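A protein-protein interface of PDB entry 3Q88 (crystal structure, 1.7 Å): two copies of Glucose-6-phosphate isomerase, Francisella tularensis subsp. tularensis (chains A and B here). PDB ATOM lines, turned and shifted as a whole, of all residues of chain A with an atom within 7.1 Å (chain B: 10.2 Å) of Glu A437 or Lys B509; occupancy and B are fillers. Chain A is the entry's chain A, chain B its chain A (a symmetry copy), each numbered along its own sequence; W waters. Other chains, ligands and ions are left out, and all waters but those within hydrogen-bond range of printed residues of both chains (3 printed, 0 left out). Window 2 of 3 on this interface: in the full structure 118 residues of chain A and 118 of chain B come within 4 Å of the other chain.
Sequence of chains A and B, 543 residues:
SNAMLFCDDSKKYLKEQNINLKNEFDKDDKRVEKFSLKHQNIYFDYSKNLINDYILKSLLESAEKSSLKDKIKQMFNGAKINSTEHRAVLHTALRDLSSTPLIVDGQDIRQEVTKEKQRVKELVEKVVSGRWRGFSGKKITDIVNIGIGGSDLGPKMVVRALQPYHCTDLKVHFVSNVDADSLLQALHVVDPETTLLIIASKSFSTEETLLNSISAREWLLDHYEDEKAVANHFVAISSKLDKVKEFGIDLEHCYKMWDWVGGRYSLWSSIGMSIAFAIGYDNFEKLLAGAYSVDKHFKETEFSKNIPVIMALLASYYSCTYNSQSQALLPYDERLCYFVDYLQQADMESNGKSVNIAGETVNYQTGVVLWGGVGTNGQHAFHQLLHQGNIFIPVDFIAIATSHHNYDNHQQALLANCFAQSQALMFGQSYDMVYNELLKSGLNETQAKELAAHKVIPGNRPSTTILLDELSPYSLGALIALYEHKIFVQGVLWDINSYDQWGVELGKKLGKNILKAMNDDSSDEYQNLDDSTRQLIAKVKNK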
ATOM      1  N   ALA A 420     -18.110  -5.892  15.284  1.00  0.00           N
ATOM      2  CA  ALA A 420     -18.634  -6.120  13.915  1.00  0.00           C
ATOM      3  C   ALA A 420     -19.496  -4.967  13.442  1.00  0.00           C
ATOM      4  O   ALA A 420     -19.524  -4.640  12.237  1.00  0.00           O
ATOM      5  CB  ALA A 420     -19.437  -7.431  13.872  1.00  0.00           C
ATOM      6  N   GLN A 423     -17.256  -2.132  12.565  1.00  0.00           N
ATOM      7  CA  GLN A 423     -16.558  -2.531  11.352  1.00  0.00           C
ATOM      8  C   GLN A 423     -17.502  -2.420  10.140  1.00  0.00           C
ATOM      9  O   GLN A 423     -17.132  -1.903   9.086  1.00  0.00           O
ATOM     10  CB  GLN A 423     -16.000  -3.931  11.492  1.00  0.00           C
ATOM     11  CG  GLN A 423     -14.988  -4.226  10.387  1.00  0.00           C
ATOM     12  CD  GLN A 423     -14.426  -5.618  10.407  1.00  0.00           C
ATOM     13  OE1 GLN A 423     -15.166  -6.618  10.488  1.00  0.00           O
ATOM     14  NE2 GLN A 423     -13.112  -5.708  10.262  1.00  0.00           N
ATOM     15  N   GLY A 428     -18.999  -1.145   4.900  1.00  0.00           N
ATOM     16  CA  GLY A 428     -20.141  -1.395   4.038  1.00  0.00           C
ATOM     17  C   GLY A 428     -19.867  -2.572   3.096  1.00  0.00           C
ATOM     18  O   GLY A 428     -18.949  -3.380   3.318  1.00  0.00           O
ATOM     19  N   GLN A 429     -20.645  -2.631   2.022  1.00  0.00           N
ATOM     20  CA  GLN A 429     -20.484  -3.647   0.990  1.00  0.00           C
ATOM     21  C   GLN A 429     -20.977  -3.085  -0.327  1.00  0.00           C
ATOM     22  O   GLN A 429     -22.060  -2.548  -0.422  1.00  0.00           O
ATOM     23  CB  GLN A 429     -21.162  -4.972   1.386  1.00  0.00           C
ATOM     24  CG  GLN A 429     -22.700  -4.978   1.479  1.00  0.00           C
ATOM     25  CD  GLN A 429     -23.300  -6.347   1.937  1.00  0.00           C
ATOM     26  OE1 GLN A 429     -22.546  -7.277   2.275  1.00  0.00           O
ATOM     27  NE2 GLN A 429     -24.665  -6.453   1.970  1.00  0.00           N
ATOM     28  N   TYR A 431     -21.905  -2.803  -4.534  1.00  0.00           N
ATOM     29  CA  TYR A 431     -22.678  -3.521  -5.565  1.00  0.00           C
ATOM     30  C   TYR A 431     -21.912  -4.736  -6.119  1.00  0.00           C
ATOM     31  O   TYR A 431     -22.455  -5.812  -6.215  1.00  0.00           O
ATOM     32  CB  TYR A 431     -23.032  -2.582  -6.710  1.00  0.00           C
ATOM     33  CG  TYR A 431     -23.910  -3.219  -7.748  1.00  0.00           C
ATOM     34  CD1 TYR A 431     -25.277  -3.110  -7.696  1.00  0.00           C
ATOM     35  CD2 TYR A 431     -23.364  -3.933  -8.796  1.00  0.00           C
ATOM     36  CE1 TYR A 431     -26.097  -3.693  -8.633  1.00  0.00           C
ATOM     37  CE2 TYR A 431     -24.181  -4.530  -9.744  1.00  0.00           C
ATOM     38  CZ  TYR A 431     -25.545  -4.404  -9.663  1.00  0.00           C
ATOM     39  OH  TYR A 431     -26.341  -5.009 -10.621  1.00  0.00           O
ATOM     40  N   ASP A 432     -20.643  -4.564  -6.468  1.00  0.00           N
ATOM     41  CA  ASP A 432     -19.847  -5.636  -7.063  1.00  0.00           C
ATOM     42  C   ASP A 432     -19.632  -6.800  -6.103  1.00  0.00           C
ATOM     43  O   ASP A 432     -19.700  -7.959  -6.506  1.00  0.00           O
ATOM     44  CB  ASP A 432     -18.487  -5.093  -7.512  1.00  0.00           C
ATOM     45  CG  ASP A 432     -18.552  -4.334  -8.816  1.00  0.00           C
ATOM     46  OD1 ASP A 432     -19.639  -4.058  -9.390  1.00  0.00           O
ATOM     47  OD2 ASP A 432     -17.453  -4.017  -9.292  1.00  0.00           O
ATOM     48  N   MET A 433     -19.402  -6.507  -4.824  1.00  0.00           N
ATOM     49  CA  MET A 433     -19.221  -7.550  -3.805  1.00  0.00           C
ATOM     50  C   MET A 433     -20.526  -8.333  -3.655  1.00  0.00           C
ATOM     51  O   MET A 433     -20.538  -9.561  -3.692  1.00  0.00           O
ATOM     52  CB  MET A 433     -18.778  -6.949  -2.466  1.00  0.00           C
ATOM     53  CG  MET A 433     -17.423  -6.199  -2.437  1.00  0.00           C
ATOM     54  SD  MET A 433     -17.311  -5.054  -0.994  1.00  0.00           S
ATOM     55  CE  MET A 433     -17.138  -6.183   0.399  1.00  0.00           C
ATOM     56  N   VAL A 434     -21.639  -7.610  -3.524  1.00  0.00           N
ATOM     57  CA  VAL A 434     -22.950  -8.236  -3.376  1.00  0.00           C
ATOM     58  C   VAL A 434     -23.355  -9.071  -4.614  1.00  0.00           C
ATOM     59  O   VAL A 434     -23.797 -10.225  -4.500  1.00  0.00           O
ATOM     60  CB  VAL A 434     -24.040  -7.187  -3.058  1.00  0.00           C
ATOM     61  CG1 VAL A 434     -25.415  -7.860  -3.134  1.00  0.00           C
ATOM     62  CG2 VAL A 434     -23.772  -6.570  -1.689  1.00  0.00           C
ATOM     63  N   TYR A 435     -23.211  -8.468  -5.779  1.00  0.00           N
ATOM     64  CA  TYR A 435     -23.555  -9.129  -7.031  1.00  0.00           C
ATOM     65  C   TYR A 435     -22.817 -10.457  -7.160  1.00  0.00           C
ATOM     66  O   TYR A 435     -23.452 -11.495  -7.438  1.00  0.00           O
ATOM     67  CB  TYR A 435     -23.220  -8.226  -8.185  1.00  0.00           C
ATOM     68  CG  TYR A 435     -23.519  -8.854  -9.516  1.00  0.00           C
ATOM     69  CD1 TYR A 435     -24.814  -8.914 -10.008  1.00  0.00           C
ATOM     70  CD2 TYR A 435     -22.495  -9.393 -10.271  1.00  0.00           C
ATOM     71  CE1 TYR A 435     -25.074  -9.498 -11.250  1.00  0.00           C
ATOM     72  CE2 TYR A 435     -22.745  -9.965 -11.496  1.00  0.00           C
ATOM     73  CZ  TYR A 435     -24.032 -10.009 -11.980  1.00  0.00           C
ATOM     74  OH  TYR A 435     -24.263 -10.609 -13.215  1.00  0.00           O
ATOM     75  N   ASN A 436     -21.510 -10.446  -6.900  1.00  0.00           N
ATOM     76  CA  ASN A 436     -20.705 -11.669  -6.984  1.00  0.00           C
ATOM     77  C   ASN A 436     -21.102 -12.716  -5.950  1.00  0.00           C
ATOM     78  O   ASN A 436     -21.172 -13.919  -6.266  1.00  0.00           O
ATOM     79  CB  ASN A 436     -19.205 -11.329  -6.957  1.00  0.00           C
ATOM     80  CG  ASN A 436     -18.738 -10.721  -8.279  1.00  0.00           C
ATOM     81  OD1 ASN A 436     -19.055 -11.232  -9.341  1.00  0.00           O
ATOM     82  ND2 ASN A 436     -18.000  -9.625  -8.218  1.00  0.00           N
ATOM     83  N   GLU A 437     -21.446 -12.248  -4.752  1.00  0.00           N
ATOM     84  CA  GLU A 437     -21.889 -13.110  -3.668  1.00  0.00           C
ATOM     85  C   GLU A 437     -23.224 -13.804  -3.997  1.00  0.00           C
ATOM     86  O   GLU A 437     -23.418 -14.974  -3.642  1.00  0.00           O
ATOM     87  CB  GLU A 437     -21.963 -12.285  -2.372  1.00  0.00           C
ATOM     88  CG  GLU A 437     -22.090 -13.079  -1.095  1.00  0.00           C
ATOM     89  CD  GLU A 437     -21.732 -12.253   0.165  1.00  0.00           C
ATOM     90  OE1 GLU A 437     -21.502 -11.015   0.056  1.00  0.00           O
ATOM     91  OE2 GLU A 437     -21.678 -12.854   1.268  1.00  0.00           O
ATOM     92  N   LEU A 438     -24.099 -13.112  -4.728  1.00  0.00           N
ATOM     93  CA  LEU A 438     -25.430 -13.629  -5.053  1.00  0.00           C
ATOM     94  C   LEU A 438     -25.329 -14.702  -6.131  1.00  0.00           C
ATOM     95  O   LEU A 438     -26.053 -15.697  -6.071  1.00  0.00           O
ATOM     96  CB  LEU A 438     -26.359 -12.517  -5.543  1.00  0.00           C
ATOM     97  CG  LEU A 438     -26.870 -11.552  -4.448  1.00  0.00           C
ATOM     98  CD1 LEU A 438     -27.695 -10.421  -5.063  1.00  0.00           C
ATOM     99  CD2 LEU A 438     -27.681 -12.315  -3.386  1.00  0.00           C
ATOM    100  N   LEU A 439     -24.451 -14.483  -7.102  1.00  0.00           N
ATOM    101  CA  LEU A 439     -24.094 -15.539  -8.072  1.00  0.00           C
ATOM    102  C   LEU A 439     -23.569 -16.808  -7.380  1.00  0.00           C
ATOM    103  O   LEU A 439     -23.984 -17.924  -7.711  1.00  0.00           O
ATOM    104  CB  LEU A 439     -23.052 -15.046  -9.057  1.00  0.00           C
ATOM    105  CG  LEU A 439     -23.461 -13.900  -9.976  1.00  0.00           C
ATOM    106  CD1 LEU A 439     -22.310 -13.565 -10.877  1.00  0.00           C
ATOM    107  CD2 LEU A 439     -24.719 -14.240 -10.790  1.00  0.00           C
ATOM    108  N   LYS A 440     -22.665 -16.648  -6.423  1.00  0.00           N
ATOM    109  CA  LYS A 440     -22.089 -17.783  -5.706  1.00  0.00           C
ATOM    110  C   LYS A 440     -23.123 -18.466  -4.799  1.00  0.00           C
ATOM    111  O   LYS A 440     -22.950 -19.624  -4.413  1.00  0.00           O
ATOM    112  CB  LYS A 440     -20.881 -17.323  -4.887  1.00  0.00           C
ATOM    113  CG  LYS A 440     -20.009 -18.442  -4.308  1.00  0.00           C
ATOM    114  CD  LYS A 440     -19.057 -17.875  -3.251  1.00  0.00           C
ATOM    115  CE  LYS A 440     -18.377 -18.974  -2.437  1.00  0.00           C
ATOM    116  NZ  LYS A 440     -17.770 -18.406  -1.205  1.00  0.00           N
ATOM    117  N   SER A 441     -24.198 -17.753  -4.457  1.00  0.00           N
ATOM    118  CA  SER A 441     -25.292 -18.317  -3.647  1.00  0.00           C
ATOM    119  C   SER A 441     -26.237 -19.201  -4.459  1.00  0.00           C
ATOM    120  O   SER A 441     -27.073 -19.902  -3.881  1.00  0.00           O
ATOM    121  CB  SER A 441     -26.134 -17.209  -3.001  1.00  0.00           C
ATOM    122  OG  SER A 441     -26.885 -16.527  -3.991  1.00  0.00           O
ATOM    123  N   GLY A 442     -26.130 -19.129  -5.784  1.00  0.00           N
ATOM    124  CA  GLY A 442     -27.008 -19.878  -6.680  1.00  0.00           C
ATOM    125  C   GLY A 442     -28.054 -19.059  -7.422  1.00  0.00           C
ATOM    126  O   GLY A 442     -28.941 -19.634  -8.056  1.00  0.00           O
ATOM    127  N   LEU A 443     -27.985 -17.730  -7.358  1.00  0.00           N
ATOM    128  CA  LEU A 443     -28.876 -16.901  -8.171  1.00  0.00           C
ATOM    129  C   LEU A 443     -28.287 -16.796  -9.569  1.00  0.00           C
ATOM    130  O   LEU A 443     -27.061 -16.809  -9.736  1.00  0.00           O
ATOM    131  CB  LEU A 443     -29.060 -15.488  -7.581  1.00  0.00           C
ATOM    132  CG  LEU A 443     -29.778 -15.287  -6.244  1.00  0.00           C
ATOM    133  CD1 LEU A 443     -29.990 -13.798  -6.045  1.00  0.00           C
ATOM    134  CD2 LEU A 443     -31.102 -16.014  -6.180  1.00  0.00           C
ATOM    135  N   ALA A 448     -29.674 -11.843  -9.602  1.00  0.00           N
ATOM    136  CA  ALA A 448     -28.612 -11.127  -8.873  1.00  0.00           C
ATOM    137  C   ALA A 448     -28.594  -9.621  -9.211  1.00  0.00           C
ATOM    138  O   ALA A 448     -28.396  -8.775  -8.325  1.00  0.00           O
ATOM    139  CB  ALA A 448     -27.239 -11.730  -9.158  1.00  0.00           C
ATOM    140  N   LYS A 455     -29.082  -4.599  -1.549  1.00  0.00           N
ATOM    141  CA  LYS A 455     -28.184  -5.091  -0.510  1.00  0.00           C
ATOM    142  C   LYS A 455     -26.937  -4.217  -0.351  1.00  0.00           C
ATOM    143  O   LYS A 455     -26.112  -4.461   0.531  1.00  0.00           O
ATOM    144  CB  LYS A 455     -27.793  -6.535  -0.760  1.00  0.00           C
ATOM    145  CG  LYS A 455     -28.998  -7.451  -0.913  1.00  0.00           C
ATOM    146  CD  LYS A 455     -28.626  -8.948  -1.042  1.00  0.00           C
ATOM    147  CE  LYS A 455     -27.824  -9.452   0.161  1.00  0.00           C
ATOM    148  NZ  LYS A 455     -27.664 -10.922   0.166  1.00  0.00           N
ATOM    149  N   GLU B 207     -28.240 -15.749  16.042  1.00  0.00           N
ATOM    150  CA  GLU B 207     -27.098 -16.006  16.937  1.00  0.00           C
ATOM    151  C   GLU B 207     -27.460 -15.919  18.400  1.00  0.00           C
ATOM    152  O   GLU B 207     -27.192 -16.822  19.202  1.00  0.00           O
ATOM    153  CB  GLU B 207     -25.971 -14.964  16.681  1.00  0.00           C
ATOM    154  CG  GLU B 207     -24.715 -15.271  17.568  1.00  0.00           C
ATOM    155  CD  GLU B 207     -23.489 -14.312  17.442  1.00  0.00           C
ATOM    156  OE1 GLU B 207     -23.642 -13.183  16.958  1.00  0.00           O
ATOM    157  OE2 GLU B 207     -22.341 -14.706  17.845  1.00  0.00           O
ATOM    158  N   TRP B 502     -32.214  -5.619   4.480  1.00  0.00           N
ATOM    159  CA  TRP B 502     -30.971  -6.153   4.010  1.00  0.00           C
ATOM    160  C   TRP B 502     -29.746  -5.560   4.680  1.00  0.00           C
ATOM    161  O   TRP B 502     -28.673  -6.186   4.668  1.00  0.00           O
ATOM    162  CB  TRP B 502     -30.852  -5.919   2.495  1.00  0.00           C
ATOM    163  CG  TRP B 502     -31.889  -6.655   1.723  1.00  0.00           C
ATOM    164  CD1 TRP B 502     -32.928  -6.127   1.031  1.00  0.00           C
ATOM    165  CD2 TRP B 502     -31.959  -8.073   1.555  1.00  0.00           C
ATOM    166  NE1 TRP B 502     -33.674  -7.151   0.448  1.00  0.00           N
ATOM    167  CE2 TRP B 502     -33.092  -8.345   0.752  1.00  0.00           C
ATOM    168  CE3 TRP B 502     -31.163  -9.140   2.013  1.00  0.00           C
ATOM    169  CZ2 TRP B 502     -33.449  -9.645   0.371  1.00  0.00           C
ATOM    170  CZ3 TRP B 502     -31.519 -10.455   1.634  1.00  0.00           C
ATOM    171  CH2 TRP B 502     -32.665 -10.679   0.815  1.00  0.00           C
ATOM    172  N   GLY B 503     -29.904  -4.412   5.311  1.00  0.00           N
ATOM    173  CA  GLY B 503     -28.785  -3.695   5.899  1.00  0.00           C
ATOM    174  C   GLY B 503     -28.129  -4.384   7.096  1.00  0.00           C
ATOM    175  O   GLY B 503     -26.987  -4.054   7.431  1.00  0.00           O
ATOM    176  N   VAL B 504     -28.826  -5.325   7.715  1.00  0.00           N
ATOM    177  CA  VAL B 504     -28.320  -6.014   8.911  1.00  0.00           C
ATOM    178  C   VAL B 504     -27.451  -7.196   8.568  1.00  0.00           C
ATOM    179  O   VAL B 504     -26.797  -7.745   9.436  1.00  0.00           O
ATOM    180  CB  VAL B 504     -29.473  -6.434   9.840  1.00  0.00           C
ATOM    181  CG1 VAL B 504     -30.343  -5.130  10.210  1.00  0.00           C
ATOM    182  CG2 VAL B 504     -30.338  -7.554   9.230  1.00  0.00           C
ATOM    183  N   GLU B 505     -27.476  -7.669   7.314  1.00  0.00           N
ATOM    184  CA  GLU B 505     -26.769  -8.893   6.980  1.00  0.00           C
ATOM    185  C   GLU B 505     -25.268  -8.829   7.166  1.00  0.00           C
ATOM    186  O   GLU B 505     -24.643  -9.802   7.621  1.00  0.00           O
ATOM    187  CB  GLU B 505     -27.040  -9.321   5.524  1.00  0.00           C
ATOM    188  CG  GLU B 505     -28.351 -10.038   5.337  1.00  0.00           C
ATOM    189  CD  GLU B 505     -28.405 -10.843   4.053  1.00  0.00           C
ATOM    190  OE1 GLU B 505     -27.697 -10.469   3.108  1.00  0.00           O
ATOM    191  OE2 GLU B 505     -29.135 -11.851   4.001  1.00  0.00           O
ATOM    192  N   LEU B 506     -24.681  -7.699   6.786  1.00  0.00           N
ATOM    193  CA  LEU B 506     -23.226  -7.543   6.773  1.00  0.00           C
ATOM    194  C   LEU B 506     -22.695  -7.703   8.192  1.00  0.00           C
ATOM    195  O   LEU B 506     -21.729  -8.392   8.401  1.00  0.00           O
ATOM    196  CB  LEU B 506     -22.870  -6.158   6.251  1.00  0.00           C
ATOM    197  CG  LEU B 506     -21.384  -5.773   6.299  1.00  0.00           C
ATOM    198  CD1 LEU B 506     -20.504  -6.809   5.500  1.00  0.00           C
ATOM    199  CD2 LEU B 506     -21.211  -4.264   5.857  1.00  0.00           C
ATOM    200  N   GLY B 507     -23.304  -7.042   9.169  1.00  0.00           N
ATOM    201  CA  GLY B 507     -22.804  -7.111  10.531  1.00  0.00           C
ATOM    202  C   GLY B 507     -22.863  -8.527  11.087  1.00  0.00           C
ATOM    203  O   GLY B 507     -22.031  -8.925  11.879  1.00  0.00           O
ATOM    204  N   LYS B 508     -23.839  -9.310  10.646  1.00  0.00           N
ATOM    205  CA  LYS B 508     -23.922 -10.721  11.084  1.00  0.00           C
ATOM    206  C   LYS B 508     -22.740 -11.557  10.541  1.00  0.00           C
ATOM    207  O   LYS B 508     -22.141 -12.318  11.299  1.00  0.00           O
ATOM    208  CB  LYS B 508     -25.264 -11.357  10.693  1.00  0.00           C
ATOM    209  CG  LYS B 508     -26.469 -10.748  11.380  1.00  0.00           C
ATOM    210  CD  LYS B 508     -27.818 -11.310  10.846  1.00  0.00           C
ATOM    211  CE  LYS B 508     -28.991 -10.618  11.509  1.00  0.00           C
ATOM    212  NZ  LYS B 508     -30.296 -11.131  10.962  1.00  0.00           N
ATOM    213  N   LYS B 509     -22.383 -11.318   9.284  1.00  0.00           N
ATOM    214  CA  LYS B 509     -21.231 -11.946   8.667  1.00  0.00           C
ATOM    215  C   LYS B 509     -19.928 -11.533   9.334  1.00  0.00           C
ATOM    216  O   LYS B 509     -19.048 -12.402   9.637  1.00  0.00           O
ATOM    217  CB  LYS B 509     -21.165 -11.571   7.158  1.00  0.00           C
ATOM    218  CG  LYS B 509     -20.041 -12.271   6.407  1.00  0.00           C
ATOM    219  CD  LYS B 509     -20.181 -12.031   4.917  1.00  0.00           C
ATOM    220  CE  LYS B 509     -19.864 -10.581   4.552  1.00  0.00           C
ATOM    221  NZ  LYS B 509     -19.931 -10.335   3.071  1.00  0.00           N
ATOM    222  N   LEU B 510     -19.779 -10.203   9.529  1.00  0.00           N
ATOM    223  CA  LEU B 510     -18.550  -9.696  10.136  1.00  0.00           C
ATOM    224  C   LEU B 510     -18.413 -10.199  11.558  1.00  0.00           C
ATOM    225  O   LEU B 510     -17.315 -10.479  12.009  1.00  0.00           O
ATOM    226  CB  LEU B 510     -18.445  -8.177  10.046  1.00  0.00           C
ATOM    227  CG  LEU B 510     -18.494  -7.550   8.653  1.00  0.00           C
ATOM    228  CD1 LEU B 510     -18.131  -6.038   8.759  1.00  0.00           C
ATOM    229  CD2 LEU B 510     -17.530  -8.307   7.697  1.00  0.00           C
ATOM    230  N   GLY B 511     -19.518 -10.410  12.231  1.00  0.00           N
ATOM    231  CA  GLY B 511     -19.501 -10.946  13.584  1.00  0.00           C
ATOM    232  C   GLY B 511     -18.960 -12.344  13.641  1.00  0.00           C
ATOM    233  O   GLY B 511     -18.149 -12.671  14.505  1.00  0.00           O
ATOM    234  N   LYS B 512     -19.366 -13.182  12.679  1.00  0.00           N
ATOM    235  CA  LYS B 512     -18.812 -14.531  12.606  1.00  0.00           C
ATOM    236  C   LYS B 512     -17.310 -14.517  12.358  1.00  0.00           C
ATOM    237  O   LYS B 512     -16.553 -15.248  13.009  1.00  0.00           O
ATOM    238  CB  LYS B 512     -19.561 -15.356  11.541  1.00  0.00           C
ATOM    239  CG  LYS B 512     -21.006 -15.668  11.916  1.00  0.00           C
ATOM    240  CD  LYS B 512     -21.613 -16.698  10.912  1.00  0.00           C
ATOM    241  CE  LYS B 512     -23.100 -16.595  10.812  1.00  0.00           C
ATOM    242  NZ  LYS B 512     -23.693 -17.536   9.783  1.00  0.00           N
ATOM    243  N   ASN B 513     -16.845 -13.635  11.463  1.00  0.00           N
ATOM    244  CA  ASN B 513     -15.434 -13.478  11.136  1.00  0.00           C
ATOM    245  C   ASN B 513     -14.593 -13.037  12.351  1.00  0.00           C
ATOM    246  O   ASN B 513     -13.520 -13.568  12.644  1.00  0.00           O
ATOM    247  CB  ASN B 513     -15.234 -12.414  10.070  1.00  0.00           C
ATOM    248  CG  ASN B 513     -15.770 -12.797   8.691  1.00  0.00           C
ATOM    249  OD1 ASN B 513     -16.134 -13.958   8.404  1.00  0.00           O
ATOM    250  ND2 ASN B 513     -15.844 -11.773   7.816  1.00  0.00           N
ATOM    251  N   ILE B 514     -15.137 -12.065  13.070  1.00  0.00           N
ATOM    252  CA  ILE B 514     -14.464 -11.521  14.245  1.00  0.00           C
ATOM    253  C   ILE B 514     -14.389 -12.558  15.340  1.00  0.00           C
ATOM    254  O   ILE B 514     -13.349 -12.683  15.986  1.00  0.00           O
ATOM    255  CB  ILE B 514     -15.144 -10.221  14.712  1.00  0.00           C
ATOM    256  CG1 ILE B 514     -14.769  -9.114  13.722  1.00  0.00           C
ATOM    257  CG2 ILE B 514     -14.745  -9.917  16.183  1.00  0.00           C
ATOM    258  CD1 ILE B 514     -15.568  -7.826  13.937  1.00  0.00           C
ATOM    259  N   LEU B 515     -15.441 -13.358  15.531  1.00  0.00           N
ATOM    260  CA  LEU B 515     -15.391 -14.392  16.557  1.00  0.00           C
ATOM    261  C   LEU B 515     -14.294 -15.407  16.208  1.00  0.00           C
ATOM    262  O   LEU B 515     -13.566 -15.841  17.086  1.00  0.00           O
ATOM    263  CB  LEU B 515     -16.755 -15.065  16.743  1.00  0.00           C
ATOM    264  CG  LEU B 515     -16.944 -15.926  17.993  1.00  0.00           C
ATOM    265  CD1 LEU B 515     -17.014 -15.024  19.182  1.00  0.00           C
ATOM    266  CD2 LEU B 515     -18.266 -16.751  17.891  1.00  0.00           C
ATOM    267  N   LYS B 516     -14.164 -15.756  14.927  1.00  0.00           N
ATOM    268  CA  LYS B 516     -13.060 -16.621  14.461  1.00  0.00           C
ATOM    269  C   LYS B 516     -11.685 -16.005  14.744  1.00  0.00           C
ATOM    270  O   LYS B 516     -10.786 -16.679  15.282  1.00  0.00           O
ATOM    271  CB  LYS B 516     -13.163 -16.895  12.959  1.00  0.00           C
ATOM    272  CG  LYS B 516     -14.093 -18.033  12.579  1.00  0.00           C
ATOM    273  CD  LYS B 516     -13.912 -18.484  11.095  1.00  0.00           C
ATOM    274  CE  LYS B 516     -15.139 -19.317  10.567  1.00  0.00           C
ATOM    275  NZ  LYS B 516     -16.497 -18.722  10.943  1.00  0.00           N
ATOM    276  N   ALA B 517     -11.520 -14.730  14.391  1.00  0.00           N
ATOM    277  CA  ALA B 517     -10.307 -13.977  14.712  1.00  0.00           C
ATOM    278  C   ALA B 517     -10.009 -13.921  16.198  1.00  0.00           C
ATOM    279  O   ALA B 517      -8.833 -13.993  16.594  1.00  0.00           O
ATOM    280  CB  ALA B 517     -10.378 -12.571  14.168  1.00  0.00           C
ATOM    281  N   GLU B 525      -9.149 -14.545   8.715  1.00  0.00           N
ATOM    282  CA  GLU B 525     -10.030 -13.558   9.373  1.00  0.00           C
ATOM    283  C   GLU B 525      -9.249 -12.539  10.228  1.00  0.00           C
ATOM    284  O   GLU B 525      -9.495 -11.330  10.131  1.00  0.00           O
ATOM    285  CB  GLU B 525     -11.073 -14.272  10.238  1.00  0.00           C
ATOM    286  CG  GLU B 525     -12.112 -15.081   9.450  1.00  0.00           C
ATOM    287  CD  GLU B 525     -11.646 -16.461   8.974  1.00  0.00           C
ATOM    288  OE1 GLU B 525     -10.601 -16.983   9.427  1.00  0.00           O
ATOM    289  OE2 GLU B 525     -12.365 -17.020   8.120  1.00  0.00           O
ATOM    290  N   LEU B 529      -8.410  -8.245   9.212  1.00  0.00           N
ATOM    291  CA  LEU B 529      -8.977  -7.159  10.055  1.00  0.00           C
ATOM    292  C   LEU B 529      -8.341  -5.790   9.804  1.00  0.00           C
ATOM    293  O   LEU B 529      -7.142  -5.654   9.554  1.00  0.00           O
ATOM    294  CB  LEU B 529      -8.817  -7.477  11.559  1.00  0.00           C
ATOM    295  CG  LEU B 529      -9.518  -8.699  12.151  1.00  0.00           C
ATOM    296  CD1 LEU B 529      -9.139  -8.914  13.629  1.00  0.00           C
ATOM    297  CD2 LEU B 529     -11.029  -8.629  11.980  1.00  0.00           C
HETATM  298  O   HOH W   1     -27.368  -7.511   2.666  1.00  0.00           O
HETATM  299  O   HOH W   2     -23.151  -9.574   3.651  1.00  0.00           O
HETATM  300  O   HOH W   3     -14.650  -9.221   9.836  1.00  0.00           O
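The side-chain amino group (NZ) of Lys A455 lies within salt-bridge range of the side-chain carboxylate (OE1) of Glu B505 (3.0 Å). The side-chain amino group (NZ) of Lys B509 is in salt-bridge range of the side-chain carboxylate (OE1) of Glu A437, 3.5 Å away.
The backbone carbonyl oxygen (O) of Lys A455 is in hydrogen-bond range of the side-chain amide nitrogen (NE2) of Gln A429 (2.9 Å).
Ala A420 touches Gly B507 (CB to O, 3.6 Å). Leu B510 touches Ala A420. Ala A420 touches Gly B511. Ala A420 touches Ile B514 (N to CD1, 3.5 Å). CD1 of Leu B510 touches OE1 of Gln A423, at 3.5 Å. Gln A423 touches Ile B514 (OE1 to CD1, 3.7 Å). Leu B529 touches Gln A423. Gly A428 touches Leu B506. Gln A429 touches Leu B506 (OE1 to CD1, 3.8 Å). Lys A455 touches Trp B502 (CE to CE3, 3.8 Å).
Glu A437 touches one residue of chain B. Of the printed residues of chain A, Lys B509 touches Glu A437 (3.5 Å). No residue of chain B comes within 4 Å of Leu A438. No residue of chain B comes within 4 Å of Ser A441. Of the printed residues of chain B, Gly A428 touches Leu B506. Printed residues of chain A within 4 Å of Leu B529: Gln A423. Of the printed residues of chain A, Leu B510 touches Ala A420 and Gln A423.
Printed residues of chain A that touch a printed residue of chain B: Ala A420, Gln A423, Gly A428, Gln A429, Glu A437 and Lys A455. Along chain A the printed residues that touch a printed residue of chain B span positions 420 to 455. Hydrophobic or aromatic side chains of chain B that line the printed part of chain A: Trp B502, Leu B506, Leu B510, Ile B514 and Leu B529.
No position is printed for both chains. Of the 12 pairs that touch across the chains among the printed residues, none has its exchanged pair printed and touching as well.
Water W3 bridges the side-chain amide oxygen of Gln A423 and the side-chain amide nitrogen of Asn B513. Water W1 lies within hydrogen-bond range of O of Trp B502 (2.7 Å), NE2 of Gln A429 (3.0 Å) and OE1 of Glu B505 (3.0 Å). Water W2 lies within hydrogen-bond range of OE1 of Gln A429 (2.7 Å) and NZ of Lys B509 (3.4 Å).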
